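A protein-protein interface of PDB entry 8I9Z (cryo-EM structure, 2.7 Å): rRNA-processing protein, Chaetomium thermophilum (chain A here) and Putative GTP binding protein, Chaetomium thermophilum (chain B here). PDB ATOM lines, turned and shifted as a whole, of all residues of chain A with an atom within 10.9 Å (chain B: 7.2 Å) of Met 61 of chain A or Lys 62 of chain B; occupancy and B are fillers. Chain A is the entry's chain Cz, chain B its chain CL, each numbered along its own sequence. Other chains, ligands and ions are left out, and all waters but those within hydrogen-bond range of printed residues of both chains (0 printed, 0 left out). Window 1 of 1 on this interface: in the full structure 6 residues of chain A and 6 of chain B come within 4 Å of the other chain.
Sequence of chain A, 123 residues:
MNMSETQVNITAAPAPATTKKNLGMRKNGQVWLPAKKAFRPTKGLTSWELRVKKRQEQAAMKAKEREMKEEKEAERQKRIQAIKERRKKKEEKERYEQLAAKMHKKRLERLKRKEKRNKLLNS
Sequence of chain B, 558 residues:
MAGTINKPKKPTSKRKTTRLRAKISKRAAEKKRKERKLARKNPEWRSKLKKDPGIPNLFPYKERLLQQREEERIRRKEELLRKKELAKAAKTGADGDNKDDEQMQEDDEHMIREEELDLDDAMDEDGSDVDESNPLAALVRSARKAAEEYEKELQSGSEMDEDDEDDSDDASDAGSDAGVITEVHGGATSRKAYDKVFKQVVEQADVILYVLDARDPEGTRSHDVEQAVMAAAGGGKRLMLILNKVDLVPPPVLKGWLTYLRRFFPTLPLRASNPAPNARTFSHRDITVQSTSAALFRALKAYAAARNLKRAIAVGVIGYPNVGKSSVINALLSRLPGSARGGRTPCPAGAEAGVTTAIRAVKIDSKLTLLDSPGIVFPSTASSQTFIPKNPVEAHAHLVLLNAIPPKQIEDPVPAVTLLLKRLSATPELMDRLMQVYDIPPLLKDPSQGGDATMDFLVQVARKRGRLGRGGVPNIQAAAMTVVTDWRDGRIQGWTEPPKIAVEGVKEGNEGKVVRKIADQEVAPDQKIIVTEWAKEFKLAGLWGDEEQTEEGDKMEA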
ATOM      1  N   LYS A  53     -16.197  -9.681  21.738  1.00  0.00           N
ATOM      2  CA  LYS A  53     -17.101  -8.750  21.079  1.00  0.00           C
ATOM      3  C   LYS A  53     -16.733  -8.599  19.610  1.00  0.00           C
ATOM      4  O   LYS A  53     -17.609  -8.546  18.741  1.00  0.00           O
ATOM      5  CB  LYS A  53     -17.072  -7.400  21.794  1.00  0.00           C
ATOM      6  CG  LYS A  53     -18.083  -6.400  21.278  1.00  0.00           C
ATOM      7  CD  LYS A  53     -17.601  -4.973  21.479  1.00  0.00           C
ATOM      8  CE  LYS A  53     -16.323  -4.705  20.701  1.00  0.00           C
ATOM      9  NZ  LYS A  53     -16.528  -4.837  19.232  1.00  0.00           N
ATOM     10  N   LYS A  54     -15.435  -8.548  19.312  1.00  0.00           N
ATOM     11  CA  LYS A  54     -14.984  -8.477  17.929  1.00  0.00           C
ATOM     12  C   LYS A  54     -15.120  -9.814  17.214  1.00  0.00           C
ATOM     13  O   LYS A  54     -15.211  -9.842  15.982  1.00  0.00           O
ATOM     14  CB  LYS A  54     -13.532  -8.005  17.872  1.00  0.00           C
ATOM     15  CG  LYS A  54     -13.251  -6.987  16.780  1.00  0.00           C
ATOM     16  CD  LYS A  54     -14.201  -5.803  16.864  1.00  0.00           C
ATOM     17  CE  LYS A  54     -13.657  -4.608  16.098  1.00  0.00           C
ATOM     18  NZ  LYS A  54     -13.805  -3.341  16.867  1.00  0.00           N
ATOM     19  N   ARG A  55     -15.109 -10.919  17.961  1.00  0.00           N
ATOM     20  CA  ARG A  55     -15.300 -12.233  17.355  1.00  0.00           C
ATOM     21  C   ARG A  55     -16.700 -12.378  16.777  1.00  0.00           C
ATOM     22  O   ARG A  55     -16.875 -12.932  15.686  1.00  0.00           O
ATOM     23  CB  ARG A  55     -15.033 -13.326  18.387  1.00  0.00           C
ATOM     24  CG  ARG A  55     -13.783 -14.137  18.129  1.00  0.00           C
ATOM     25  CD  ARG A  55     -13.321 -14.817  19.399  1.00  0.00           C
ATOM     26  NE  ARG A  55     -13.697 -16.223  19.452  1.00  0.00           N
ATOM     27  CZ  ARG A  55     -13.728 -16.939  20.566  1.00  0.00           C
ATOM     28  NH1 ARG A  55     -13.413 -16.411  21.736  1.00  0.00           N
ATOM     29  NH2 ARG A  55     -14.079 -18.219  20.503  1.00  0.00           N
ATOM     30  N   GLN A  56     -17.711 -11.893  17.501  1.00  0.00           N
ATOM     31  CA  GLN A  56     -19.073 -11.915  16.983  1.00  0.00           C
ATOM     32  C   GLN A  56     -19.229 -10.956  15.811  1.00  0.00           C
ATOM     33  O   GLN A  56     -19.953 -11.252  14.853  1.00  0.00           O
ATOM     34  CB  GLN A  56     -20.062 -11.563  18.090  1.00  0.00           C
ATOM     35  CG  GLN A  56     -20.568 -12.756  18.870  1.00  0.00           C
ATOM     36  CD  GLN A  56     -20.049 -12.778  20.288  1.00  0.00           C
ATOM     37  OE1 GLN A  56     -20.145 -11.788  21.010  1.00  0.00           O
ATOM     38  NE2 GLN A  56     -19.494 -13.912  20.697  1.00  0.00           N
ATOM     39  N   GLU A  57     -18.570  -9.798  15.878  1.00  0.00           N
ATOM     40  CA  GLU A  57     -18.643  -8.837  14.784  1.00  0.00           C
ATOM     41  C   GLU A  57     -17.964  -9.372  13.532  1.00  0.00           C
ATOM     42  O   GLU A  57     -18.441  -9.145  12.417  1.00  0.00           O
ATOM     43  CB  GLU A  57     -18.021  -7.507  15.204  1.00  0.00           C
ATOM     44  CG  GLU A  57     -18.828  -6.739  16.229  1.00  0.00           C
ATOM     45  CD  GLU A  57     -18.347  -5.312  16.397  1.00  0.00           C
ATOM     46  OE1 GLU A  57     -17.477  -4.880  15.611  1.00  0.00           O
ATOM     47  OE2 GLU A  57     -18.841  -4.620  17.311  1.00  0.00           O
ATOM     48  N   GLN A  58     -16.849 -10.084  13.697  1.00  0.00           N
ATOM     49  CA  GLN A  58     -16.176 -10.681  12.548  1.00  0.00           C
ATOM     50  C   GLN A  58     -16.986 -11.833  11.966  1.00  0.00           C
ATOM     51  O   GLN A  58     -16.927 -12.090  10.759  1.00  0.00           O
ATOM     52  CB  GLN A  58     -14.779 -11.156  12.944  1.00  0.00           C
ATOM     53  CG  GLN A  58     -13.736 -11.008  11.848  1.00  0.00           C
ATOM     54  CD  GLN A  58     -13.161  -9.608  11.773  1.00  0.00           C
ATOM     55  OE1 GLN A  58     -12.912  -8.972  12.798  1.00  0.00           O
ATOM     56  NE2 GLN A  58     -12.946  -9.119  10.557  1.00  0.00           N
ATOM     57  N   ALA A  59     -17.740 -12.541  12.811  1.00  0.00           N
ATOM     58  CA  ALA A  59     -18.534 -13.670  12.333  1.00  0.00           C
ATOM     59  C   ALA A  59     -19.694 -13.210  11.460  1.00  0.00           C
ATOM     60  O   ALA A  59     -19.968 -13.811  10.416  1.00  0.00           O
ATOM     61  CB  ALA A  59     -19.046 -14.489  13.517  1.00  0.00           C
ATOM     62  N   ALA A  60     -20.393 -12.152  11.875  1.00  0.00           N
ATOM     63  CA  ALA A  60     -21.467 -11.608  11.051  1.00  0.00           C
ATOM     64  C   ALA A  60     -20.914 -10.935   9.804  1.00  0.00           C
ATOM     65  O   ALA A  60     -21.540 -10.969   8.738  1.00  0.00           O
ATOM     66  CB  ALA A  60     -22.308 -10.627  11.865  1.00  0.00           C
ATOM     67  N   MET A  61     -19.745 -10.304   9.927  1.00  0.00           N
ATOM     68  CA  MET A  61     -19.061  -9.728   8.773  1.00  0.00           C
ATOM     69  C   MET A  61     -18.661 -10.803   7.773  1.00  0.00           C
ATOM     70  O   MET A  61     -18.803 -10.612   6.560  1.00  0.00           O
ATOM     71  CB  MET A  61     -17.843  -8.948   9.260  1.00  0.00           C
ATOM     72  CG  MET A  61     -17.240  -7.956   8.298  1.00  0.00           C
ATOM     73  SD  MET A  61     -15.918  -8.726   7.355  1.00  0.00           S
ATOM     74  CE  MET A  61     -14.561  -7.652   7.810  1.00  0.00           C
ATOM     75  N   LYS A  62     -18.159 -11.938   8.260  1.00  0.00           N
ATOM     76  CA  LYS A  62     -17.830 -13.041   7.364  1.00  0.00           C
ATOM     77  C   LYS A  62     -19.090 -13.703   6.825  1.00  0.00           C
ATOM     78  O   LYS A  62     -19.084 -14.244   5.712  1.00  0.00           O
ATOM     79  CB  LYS A  62     -16.949 -14.060   8.084  1.00  0.00           C
ATOM     80  CG  LYS A  62     -15.491 -13.648   8.199  1.00  0.00           C
ATOM     81  CD  LYS A  62     -14.623 -14.805   8.664  1.00  0.00           C
ATOM     82  CE  LYS A  62     -13.162 -14.400   8.745  1.00  0.00           C
ATOM     83  NZ  LYS A  62     -12.284 -15.561   9.052  1.00  0.00           N
ATOM     84  N   ALA A  63     -20.172 -13.693   7.609  1.00  0.00           N
ATOM     85  CA  ALA A  63     -21.448 -14.192   7.108  1.00  0.00           C
ATOM     86  C   ALA A  63     -21.979 -13.309   5.987  1.00  0.00           C
ATOM     87  O   ALA A  63     -22.520 -13.811   4.994  1.00  0.00           O
ATOM     88  CB  ALA A  63     -22.463 -14.281   8.247  1.00  0.00           C
ATOM     89  N   LYS A  64     -21.832 -11.989   6.127  1.00  0.00           N
ATOM     90  CA  LYS A  64     -22.248 -11.078   5.067  1.00  0.00           C
ATOM     91  C   LYS A  64     -21.341 -11.198   3.851  1.00  0.00           C
ATOM     92  O   LYS A  64     -21.769 -10.940   2.722  1.00  0.00           O
ATOM     93  CB  LYS A  64     -22.262  -9.639   5.582  1.00  0.00           C
ATOM     94  CG  LYS A  64     -23.409  -9.319   6.520  1.00  0.00           C
ATOM     95  CD  LYS A  64     -23.301  -7.895   7.041  1.00  0.00           C
ATOM     96  CE  LYS A  64     -24.450  -7.554   7.976  1.00  0.00           C
ATOM     97  NZ  LYS A  64     -24.325  -6.176   8.522  1.00  0.00           N
ATOM     98  N   GLU A  65     -20.078 -11.575   4.065  1.00  0.00           N
ATOM     99  CA  GLU A  65     -19.156 -11.781   2.952  1.00  0.00           C
ATOM    100  C   GLU A  65     -19.593 -12.951   2.080  1.00  0.00           C
ATOM    101  O   GLU A  65     -19.548 -12.876   0.848  1.00  0.00           O
ATOM    102  CB  GLU A  65     -17.741 -12.015   3.485  1.00  0.00           C
ATOM    103  CG  GLU A  65     -16.956 -10.752   3.786  1.00  0.00           C
ATOM    104  CD  GLU A  65     -15.582 -11.053   4.356  1.00  0.00           C
ATOM    105  OE1 GLU A  65     -15.363 -12.196   4.806  1.00  0.00           O
ATOM    106  OE2 GLU A  65     -14.722 -10.148   4.354  1.00  0.00           O
ATOM    107  N   ARG A  66     -20.022 -14.048   2.710  1.00  0.00           N
ATOM    108  CA  ARG A  66     -20.391 -15.240   1.955  1.00  0.00           C
ATOM    109  C   ARG A  66     -21.719 -15.054   1.232  1.00  0.00           C
ATOM    110  O   ARG A  66     -21.937 -15.637   0.164  1.00  0.00           O
ATOM    111  CB  ARG A  66     -20.456 -16.451   2.886  1.00  0.00           C
ATOM    112  CG  ARG A  66     -19.110 -16.889   3.442  1.00  0.00           C
ATOM    113  CD  ARG A  66     -19.268 -18.035   4.429  1.00  0.00           C
ATOM    114  NE  ARG A  66     -17.999 -18.415   5.037  1.00  0.00           N
ATOM    115  CZ  ARG A  66     -17.877 -19.260   6.051  1.00  0.00           C
ATOM    116  NH1 ARG A  66     -18.932 -19.837   6.603  1.00  0.00           N
ATOM    117  NH2 ARG A  66     -16.664 -19.534   6.525  1.00  0.00           N
ATOM    118  N   GLU A  67     -22.621 -14.252   1.802  1.00  0.00           N
ATOM    119  CA  GLU A  67     -23.954 -14.106   1.225  1.00  0.00           C
ATOM    120  C   GLU A  67     -23.912 -13.319  -0.079  1.00  0.00           C
ATOM    121  O   GLU A  67     -24.558 -13.694  -1.064  1.00  0.00           O
ATOM    122  CB  GLU A  67     -24.891 -13.437   2.232  1.00  0.00           C
ATOM    123  CG  GLU A  67     -25.366 -14.362   3.341  1.00  0.00           C
ATOM    124  CD  GLU A  67     -26.298 -13.673   4.318  1.00  0.00           C
ATOM    125  OE1 GLU A  67     -26.413 -12.431   4.258  1.00  0.00           O
ATOM    126  OE2 GLU A  67     -26.918 -14.375   5.146  1.00  0.00           O
ATOM    127  N   MET A  68     -23.158 -12.218  -0.105  1.00  0.00           N
ATOM    128  CA  MET A  68     -23.051 -11.431  -1.331  1.00  0.00           C
ATOM    129  C   MET A  68     -22.218 -12.153  -2.381  1.00  0.00           C
ATOM    130  O   MET A  68     -22.440 -11.976  -3.584  1.00  0.00           O
ATOM    131  CB  MET A  68     -22.466 -10.052  -1.030  1.00  0.00           C
ATOM    132  CG  MET A  68     -23.063  -9.377   0.192  1.00  0.00           C
ATOM    133  SD  MET A  68     -22.871  -7.586   0.169  1.00  0.00           S
ATOM    134  CE  MET A  68     -23.276  -7.223  -1.537  1.00  0.00           C
ATOM    135  N   LYS A  69     -21.249 -12.961  -1.949  1.00  0.00           N
ATOM    136  CA  LYS A  69     -20.495 -13.778  -2.895  1.00  0.00           C
ATOM    137  C   LYS A  69     -21.372 -14.864  -3.503  1.00  0.00           C
ATOM    138  O   LYS A  69     -21.259 -15.166  -4.696  1.00  0.00           O
ATOM    139  CB  LYS A  69     -19.275 -14.391  -2.206  1.00  0.00           C
ATOM    140  CG  LYS A  69     -18.102 -13.435  -2.058  1.00  0.00           C
ATOM    141  CD  LYS A  69     -16.932 -14.103  -1.353  1.00  0.00           C
ATOM    142  CE  LYS A  69     -15.713 -13.195  -1.330  1.00  0.00           C
ATOM    143  NZ  LYS A  69     -14.568 -13.823  -0.614  1.00  0.00           N
ATOM    144  N   LYS A  72     -23.812 -13.102  -5.986  1.00  0.00           N
ATOM    145  CA  LYS A  72     -23.147 -12.722  -7.228  1.00  0.00           C
ATOM    146  C   LYS A  72     -22.822 -13.943  -8.078  1.00  0.00           C
ATOM    147  O   LYS A  72     -22.936 -13.899  -9.308  1.00  0.00           O
ATOM    148  CB  LYS A  72     -21.877 -11.929  -6.921  1.00  0.00           C
ATOM    149  CG  LYS A  72     -22.127 -10.489  -6.507  1.00  0.00           C
ATOM    150  CD  LYS A  72     -20.829  -9.792  -6.131  1.00  0.00           C
ATOM    151  CE  LYS A  72     -21.067  -8.336  -5.767  1.00  0.00           C
ATOM    152  NZ  LYS A  72     -19.806  -7.654  -5.365  1.00  0.00           N
ATOM    153  N   PRO B  53      -9.257  -7.572  -5.005  1.00  0.00           N
ATOM    154  CA  PRO B  53      -9.262  -8.415  -3.799  1.00  0.00           C
ATOM    155  C   PRO B  53     -10.344  -8.050  -2.797  1.00  0.00           C
ATOM    156  O   PRO B  53     -10.699  -8.889  -1.961  1.00  0.00           O
ATOM    157  CB  PRO B  53      -7.859  -8.200  -3.212  1.00  0.00           C
ATOM    158  CG  PRO B  53      -7.042  -7.680  -4.351  1.00  0.00           C
ATOM    159  CD  PRO B  53      -7.978  -6.868  -5.181  1.00  0.00           C
ATOM    160  N   GLY B  54     -10.878  -6.838  -2.854  1.00  0.00           N
ATOM    161  CA  GLY B  54     -11.948  -6.422  -1.972  1.00  0.00           C
ATOM    162  C   GLY B  54     -11.434  -5.649  -0.776  1.00  0.00           C
ATOM    163  O   GLY B  54     -10.238  -5.387  -0.619  1.00  0.00           O
ATOM    164  N   ILE B  55     -12.380  -5.265   0.069  1.00  0.00           N
ATOM    165  CA  ILE B  55     -12.052  -4.558   1.311  1.00  0.00           C
ATOM    166  C   ILE B  55     -11.333  -5.518   2.251  1.00  0.00           C
ATOM    167  O   ILE B  55     -11.747  -6.685   2.364  1.00  0.00           O
ATOM    168  CB  ILE B  55     -13.326  -4.002   1.951  1.00  0.00           C
ATOM    169  CG1 ILE B  55     -14.222  -3.375   0.888  1.00  0.00           C
ATOM    170  CG2 ILE B  55     -13.001  -2.967   3.013  1.00  0.00           C
ATOM    171  CD1 ILE B  55     -15.623  -3.097   1.365  1.00  0.00           C
ATOM    172  N   PRO B  56     -10.252  -5.100   2.908  1.00  0.00           N
ATOM    173  CA  PRO B  56      -9.567  -5.998   3.841  1.00  0.00           C
ATOM    174  C   PRO B  56     -10.429  -6.332   5.045  1.00  0.00           C
ATOM    175  O   PRO B  56     -11.288  -5.554   5.461  1.00  0.00           O
ATOM    176  CB  PRO B  56      -8.324  -5.203   4.255  1.00  0.00           C
ATOM    177  CG  PRO B  56      -8.139  -4.200   3.184  1.00  0.00           C
ATOM    178  CD  PRO B  56      -9.502  -3.851   2.706  1.00  0.00           C
ATOM    179  N   ASN B  57     -10.195  -7.525   5.593  1.00  0.00           N
ATOM    180  CA  ASN B  57     -10.967  -7.975   6.743  1.00  0.00           C
ATOM    181  C   ASN B  57     -10.629  -7.178   7.994  1.00  0.00           C
ATOM    182  O   ASN B  57     -11.479  -7.021   8.875  1.00  0.00           O
ATOM    183  CB  ASN B  57     -10.728  -9.464   6.983  1.00  0.00           C
ATOM    184  CG  ASN B  57     -11.337 -10.326   5.905  1.00  0.00           C
ATOM    185  OD1 ASN B  57     -11.602  -9.860   4.800  1.00  0.00           O
ATOM    186  ND2 ASN B  57     -11.562 -11.596   6.218  1.00  0.00           N
ATOM    187  N   LEU B  58      -9.406  -6.669   8.090  1.00  0.00           N
ATOM    188  CA  LEU B  58      -8.995  -5.888   9.246  1.00  0.00           C
ATOM    189  C   LEU B  58      -9.482  -4.450   9.185  1.00  0.00           C
ATOM    190  O   LEU B  58      -9.279  -3.706  10.149  1.00  0.00           O
ATOM    191  CB  LEU B  58      -7.471  -5.922   9.382  1.00  0.00           C
ATOM    192  CG  LEU B  58      -6.845  -7.285   9.687  1.00  0.00           C
ATOM    193  CD1 LEU B  58      -5.421  -7.120  10.180  1.00  0.00           C
ATOM    194  CD2 LEU B  58      -7.671  -8.060  10.708  1.00  0.00           C
ATOM    195  N   PHE B  59     -10.099  -4.045   8.083  1.00  0.00           N
ATOM    196  CA  PHE B  59     -10.744  -2.745   8.003  1.00  0.00           C
ATOM    197  C   PHE B  59     -11.922  -2.719   8.964  1.00  0.00           C
ATOM    198  O   PHE B  59     -12.801  -3.586   8.873  1.00  0.00           O
ATOM    199  CB  PHE B  59     -11.207  -2.474   6.577  1.00  0.00           C
ATOM    200  CG  PHE B  59     -11.563  -1.041   6.314  1.00  0.00           C
ATOM    201  CD1 PHE B  59     -10.621  -0.039   6.460  1.00  0.00           C
ATOM    202  CD2 PHE B  59     -12.839  -0.698   5.907  1.00  0.00           C
ATOM    203  CE1 PHE B  59     -10.951   1.279   6.215  1.00  0.00           C
ATOM    204  CE2 PHE B  59     -13.173   0.616   5.659  1.00  0.00           C
ATOM    205  CZ  PHE B  59     -12.227   1.605   5.814  1.00  0.00           C
ATOM    206  N   PRO B  60     -11.977  -1.768   9.899  1.00  0.00           N
ATOM    207  CA  PRO B  60     -13.022  -1.816  10.932  1.00  0.00           C
ATOM    208  C   PRO B  60     -14.418  -1.513  10.423  1.00  0.00           C
ATOM    209  O   PRO B  60     -15.387  -1.818  11.127  1.00  0.00           O
ATOM    210  CB  PRO B  60     -12.557  -0.766  11.949  1.00  0.00           C
ATOM    211  CG  PRO B  60     -11.695   0.154  11.172  1.00  0.00           C
ATOM    212  CD  PRO B  60     -11.024  -0.671  10.123  1.00  0.00           C
ATOM    213  N   TYR B  61     -14.561  -0.943   9.230  1.00  0.00           N
ATOM    214  CA  TYR B  61     -15.866  -0.544   8.722  1.00  0.00           C
ATOM    215  C   TYR B  61     -16.176  -1.197   7.383  1.00  0.00           C
ATOM    216  O   TYR B  61     -16.715  -0.555   6.482  1.00  0.00           O
ATOM    217  CB  TYR B  61     -15.951   0.976   8.617  1.00  0.00           C
ATOM    218  CG  TYR B  61     -15.844   1.612   9.972  1.00  0.00           C
ATOM    219  CD1 TYR B  61     -16.593   1.132  11.036  1.00  0.00           C
ATOM    220  CD2 TYR B  61     -14.966   2.657  10.204  1.00  0.00           C
ATOM    221  CE1 TYR B  61     -16.485   1.688  12.284  1.00  0.00           C
ATOM    222  CE2 TYR B  61     -14.854   3.219  11.450  1.00  0.00           C
ATOM    223  CZ  TYR B  61     -15.615   2.730  12.482  1.00  0.00           C
ATOM    224  OH  TYR B  61     -15.509   3.281  13.731  1.00  0.00           O
ATOM    225  N   LYS B  62     -15.832  -2.479   7.234  1.00  0.00           N
ATOM    226  CA  LYS B  62     -16.266  -3.214   6.052  1.00  0.00           C
ATOM    227  C   LYS B  62     -17.765  -3.467   6.086  1.00  0.00           C
ATOM    228  O   LYS B  62     -18.406  -3.557   5.032  1.00  0.00           O
ATOM    229  CB  LYS B  62     -15.497  -4.533   5.931  1.00  0.00           C
ATOM    230  CG  LYS B  62     -15.714  -5.263   4.608  1.00  0.00           C
ATOM    231  CD  LYS B  62     -14.764  -6.429   4.432  1.00  0.00           C
ATOM    232  CE  LYS B  62     -14.976  -7.128   3.106  1.00  0.00           C
ATOM    233  NZ  LYS B  62     -13.983  -8.217   2.905  1.00  0.00           N
ATOM    234  N   GLU B  63     -18.344  -3.566   7.284  1.00  0.00           N
ATOM    235  CA  GLU B  63     -19.771  -3.835   7.408  1.00  0.00           C
ATOM    236  C   GLU B  63     -20.606  -2.643   6.955  1.00  0.00           C
ATOM    237  O   GLU B  63     -21.594  -2.808   6.230  1.00  0.00           O
ATOM    238  CB  GLU B  63     -20.105  -4.214   8.851  1.00  0.00           C
ATOM    239  CG  GLU B  63     -20.350  -5.697   9.061  1.00  0.00           C
ATOM    240  CD  GLU B  63     -21.294  -5.972  10.214  1.00  0.00           C
ATOM    241  OE1 GLU B  63     -22.330  -5.283  10.316  1.00  0.00           O
ATOM    242  OE2 GLU B  63     -21.000  -6.880  11.020  1.00  0.00           O
ATOM    243  N   ARG B  64     -20.230  -1.432   7.372  1.00  0.00           N
ATOM    244  CA  ARG B  64     -20.992  -0.265   6.944  1.00  0.00           C
ATOM    245  C   ARG B  64     -20.667   0.120   5.507  1.00  0.00           C
ATOM    246  O   ARG B  64     -21.431   0.858   4.878  1.00  0.00           O
ATOM    247  CB  ARG B  64     -20.747   0.918   7.879  1.00  0.00           C
ATOM    248  CG  ARG B  64     -19.439   1.642   7.653  1.00  0.00           C
ATOM    249  CD  ARG B  64     -19.364   2.921   8.470  1.00  0.00           C
ATOM    250  NE  ARG B  64     -19.348   2.657   9.904  1.00  0.00           N
ATOM    251  CZ  ARG B  64     -20.350   2.932  10.726  1.00  0.00           C
ATOM    252  NH1 ARG B  64     -21.470   3.485  10.289  1.00  0.00           N
ATOM    253  NH2 ARG B  64     -20.227   2.642  12.018  1.00  0.00           N
ATOM    254  N   LEU B  65     -19.542  -0.358   4.974  1.00  0.00           N
ATOM    255  CA  LEU B  65     -19.245  -0.134   3.564  1.00  0.00           C
ATOM    256  C   LEU B  65     -20.021  -1.102   2.683  1.00  0.00           C
ATOM    257  O   LEU B  65     -20.404  -0.757   1.558  1.00  0.00           O
ATOM    258  CB  LEU B  65     -17.743  -0.268   3.316  1.00  0.00           C
ATOM    259  CG  LEU B  65     -16.962   1.032   3.138  1.00  0.00           C
ATOM    260  CD1 LEU B  65     -17.358   1.710   1.838  1.00  0.00           C
ATOM    261  CD2 LEU B  65     -17.180   1.963   4.322  1.00  0.00           C
ATOM    262  N   LEU B  66     -20.250  -2.324   3.170  1.00  0.00           N
ATOM    263  CA  LEU B  66     -21.020  -3.294   2.400  1.00  0.00           C
ATOM    264  C   LEU B  66     -22.486  -2.892   2.312  1.00  0.00           C
ATOM    265  O   LEU B  66     -23.121  -3.077   1.267  1.00  0.00           O
ATOM    266  CB  LEU B  66     -20.881  -4.686   3.011  1.00  0.00           C
ATOM    267  CG  LEU B  66     -19.632  -5.480   2.622  1.00  0.00           C
ATOM    268  CD1 LEU B  66     -19.498  -6.724   3.484  1.00  0.00           C
ATOM    269  CD2 LEU B  66     -19.674  -5.848   1.150  1.00  0.00           C
ATOM    270  N   GLN B  67     -23.041  -2.336   3.392  1.00  0.00           N
ATOM    271  CA  GLN B  67     -24.434  -1.905   3.356  1.00  0.00           C
ATOM    272  C   GLN B  67     -24.608  -0.682   2.464  1.00  0.00           C
ATOM    273  O   GLN B  67     -25.688  -0.462   1.905  1.00  0.00           O
ATOM    274  CB  GLN B  67     -24.946  -1.668   4.785  1.00  0.00           C
ATOM    275  CG  GLN B  67     -24.426  -0.444   5.563  1.00  0.00           C
ATOM    276  CD  GLN B  67     -25.071   0.880   5.175  1.00  0.00           C
ATOM    277  OE1 GLN B  67     -26.221   0.919   4.736  1.00  0.00           O
ATOM    278  NE2 GLN B  67     -24.330   1.970   5.340  1.00  0.00           N
ATOM    279  N   GLN B  68     -23.557   0.127   2.321  1.00  0.00           N
ATOM    280  CA  GLN B  68     -23.575   1.205   1.339  1.00  0.00           C
ATOM    281  C   GLN B  68     -23.584   0.645  -0.076  1.00  0.00           C
ATOM    282  O   GLN B  68     -24.176   1.231  -0.990  1.00  0.00           O
ATOM    283  CB  GLN B  68     -22.374   2.127   1.548  1.00  0.00           C
ATOM    284  CG  GLN B  68     -22.524   3.101   2.698  1.00  0.00           C
ATOM    285  CD  GLN B  68     -21.582   4.284   2.581  1.00  0.00           C
ATOM    286  OE1 GLN B  68     -20.451   4.242   3.064  1.00  0.00           O
ATOM    287  NE2 GLN B  68     -22.046   5.347   1.934  1.00  0.00           N
ATOM    288  N   ARG B  69     -22.905  -0.489  -0.280  1.00  0.00           N
ATOM    289  CA  ARG B  69     -22.940  -1.150  -1.580  1.00  0.00           C
ATOM    290  C   ARG B  69     -24.324  -1.713  -1.880  1.00  0.00           C
ATOM    291  O   ARG B  69     -24.800  -1.634  -3.018  1.00  0.00           O
ATOM    292  CB  ARG B  69     -21.895  -2.264  -1.641  1.00  0.00           C
ATOM    293  CG  ARG B  69     -20.463  -1.798  -1.821  1.00  0.00           C
ATOM    294  CD  ARG B  69     -19.538  -3.003  -1.915  1.00  0.00           C
ATOM    295  NE  ARG B  69     -18.130  -2.636  -2.003  1.00  0.00           N
ATOM    296  CZ  ARG B  69     -17.131  -3.507  -1.966  1.00  0.00           C
ATOM    297  NH1 ARG B  69     -17.350  -4.807  -1.845  1.00  0.00           N
ATOM    298  NH2 ARG B  69     -15.880  -3.066  -2.055  1.00  0.00           N
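The side-chain amino group of Lys 62 of chain B sits at hydrogen-bond distance from the backbone carbonyl oxygen of Ile 55 of chain B, at 2.8 Å.
NZ of Lys 62 of chain B sits at hydrogen-bond distance from OD1 of Asn 57 of chain B.
The side-chain carboxylate (OE2) of Glu 57 of chain A is in salt-bridge range of the side-chain amino group (NZ) of Lys 53 of chain A (3.0 Å).
The backbone carbonyl oxygen of Asn 57 of chain B sits at hydrogen-bond distance from the side-chain amide nitrogen of Gln 58 of chain A (3.1 Å).
OD1 of Asn 57 of chain B lies close to OE2 of Glu 65 of chain A (3.2 Å).
The side-chain amino group (NZ) of Lys 62 of chain B lies within salt-bridge range of the side-chain carboxylate (OE2) of Glu 65 of chain A.
NZ of Lys 64 of chain A lies within salt-bridge range of OE1 of Glu 63 of chain B, at 2.8 Å.
Met 61 of chain A touches three residues of chain B.
Lys 62 of chain B touches just these residues of chain A: Met 61 and Glu 65.
Gly 54 of chain B touches none of the printed residues of chain A.
No residue of chain A comes within 4 Å of Phe 59 of chain B.
No residue of chain A comes within 4 Å of Leu 65 of chain B.
Leu 66 of chain B touches just one residue of chain A: Met 68.
Of the printed residues of chain B, Gln 58 of chain A touches Asn 57 (3.1 Å).
Of the printed residues of chain B, Glu 65 of chain A touches Asn 57 (3.2 Å) and Lys 62 (2.5 Å).
Of the printed residues of chain B, Glu 57 of chain A touches Glu 63.
Gln 68 of chain B touches none of the printed residues of chain A.
The nearest printed residue of chain B that does not touch Met 61 of chain A is Pro 56 of chain B (4.5 Å).
Of the 18 printed residues of chain A, 6 touch a printed residue of chain B.
Printed residues of chain A that touch a printed residue of chain B: Glu 57, Gln 58, Met 61, Lys 64, Glu 65 and Met 68.
Hydrophobic or aromatic side chains of chain A that line the printed part of chain B: Met 61 and Met 68.
Of the 17 printed residues of chain B, 4 touch a printed residue of chain A.
Printed residues of chain B that touch a printed residue of chain A: Asn 57, Lys 62, Glu 63 and Leu 66.
OE2 of Glu 63 of chain B touches O of Glu 57 of chain A (3.7 Å).
Met 61 of chain A touches Asn 57 of chain B (CE to O, 3.3 Å).
Met 61 of chain A touches Lys 62 of chain B (CE to CD, 3.6 Å).
N of Met 61 of chain A touches OE2 of Glu 63 of chain B, 3.8 Å away.
Met 68 of chain A touches Leu 66 of chain B.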
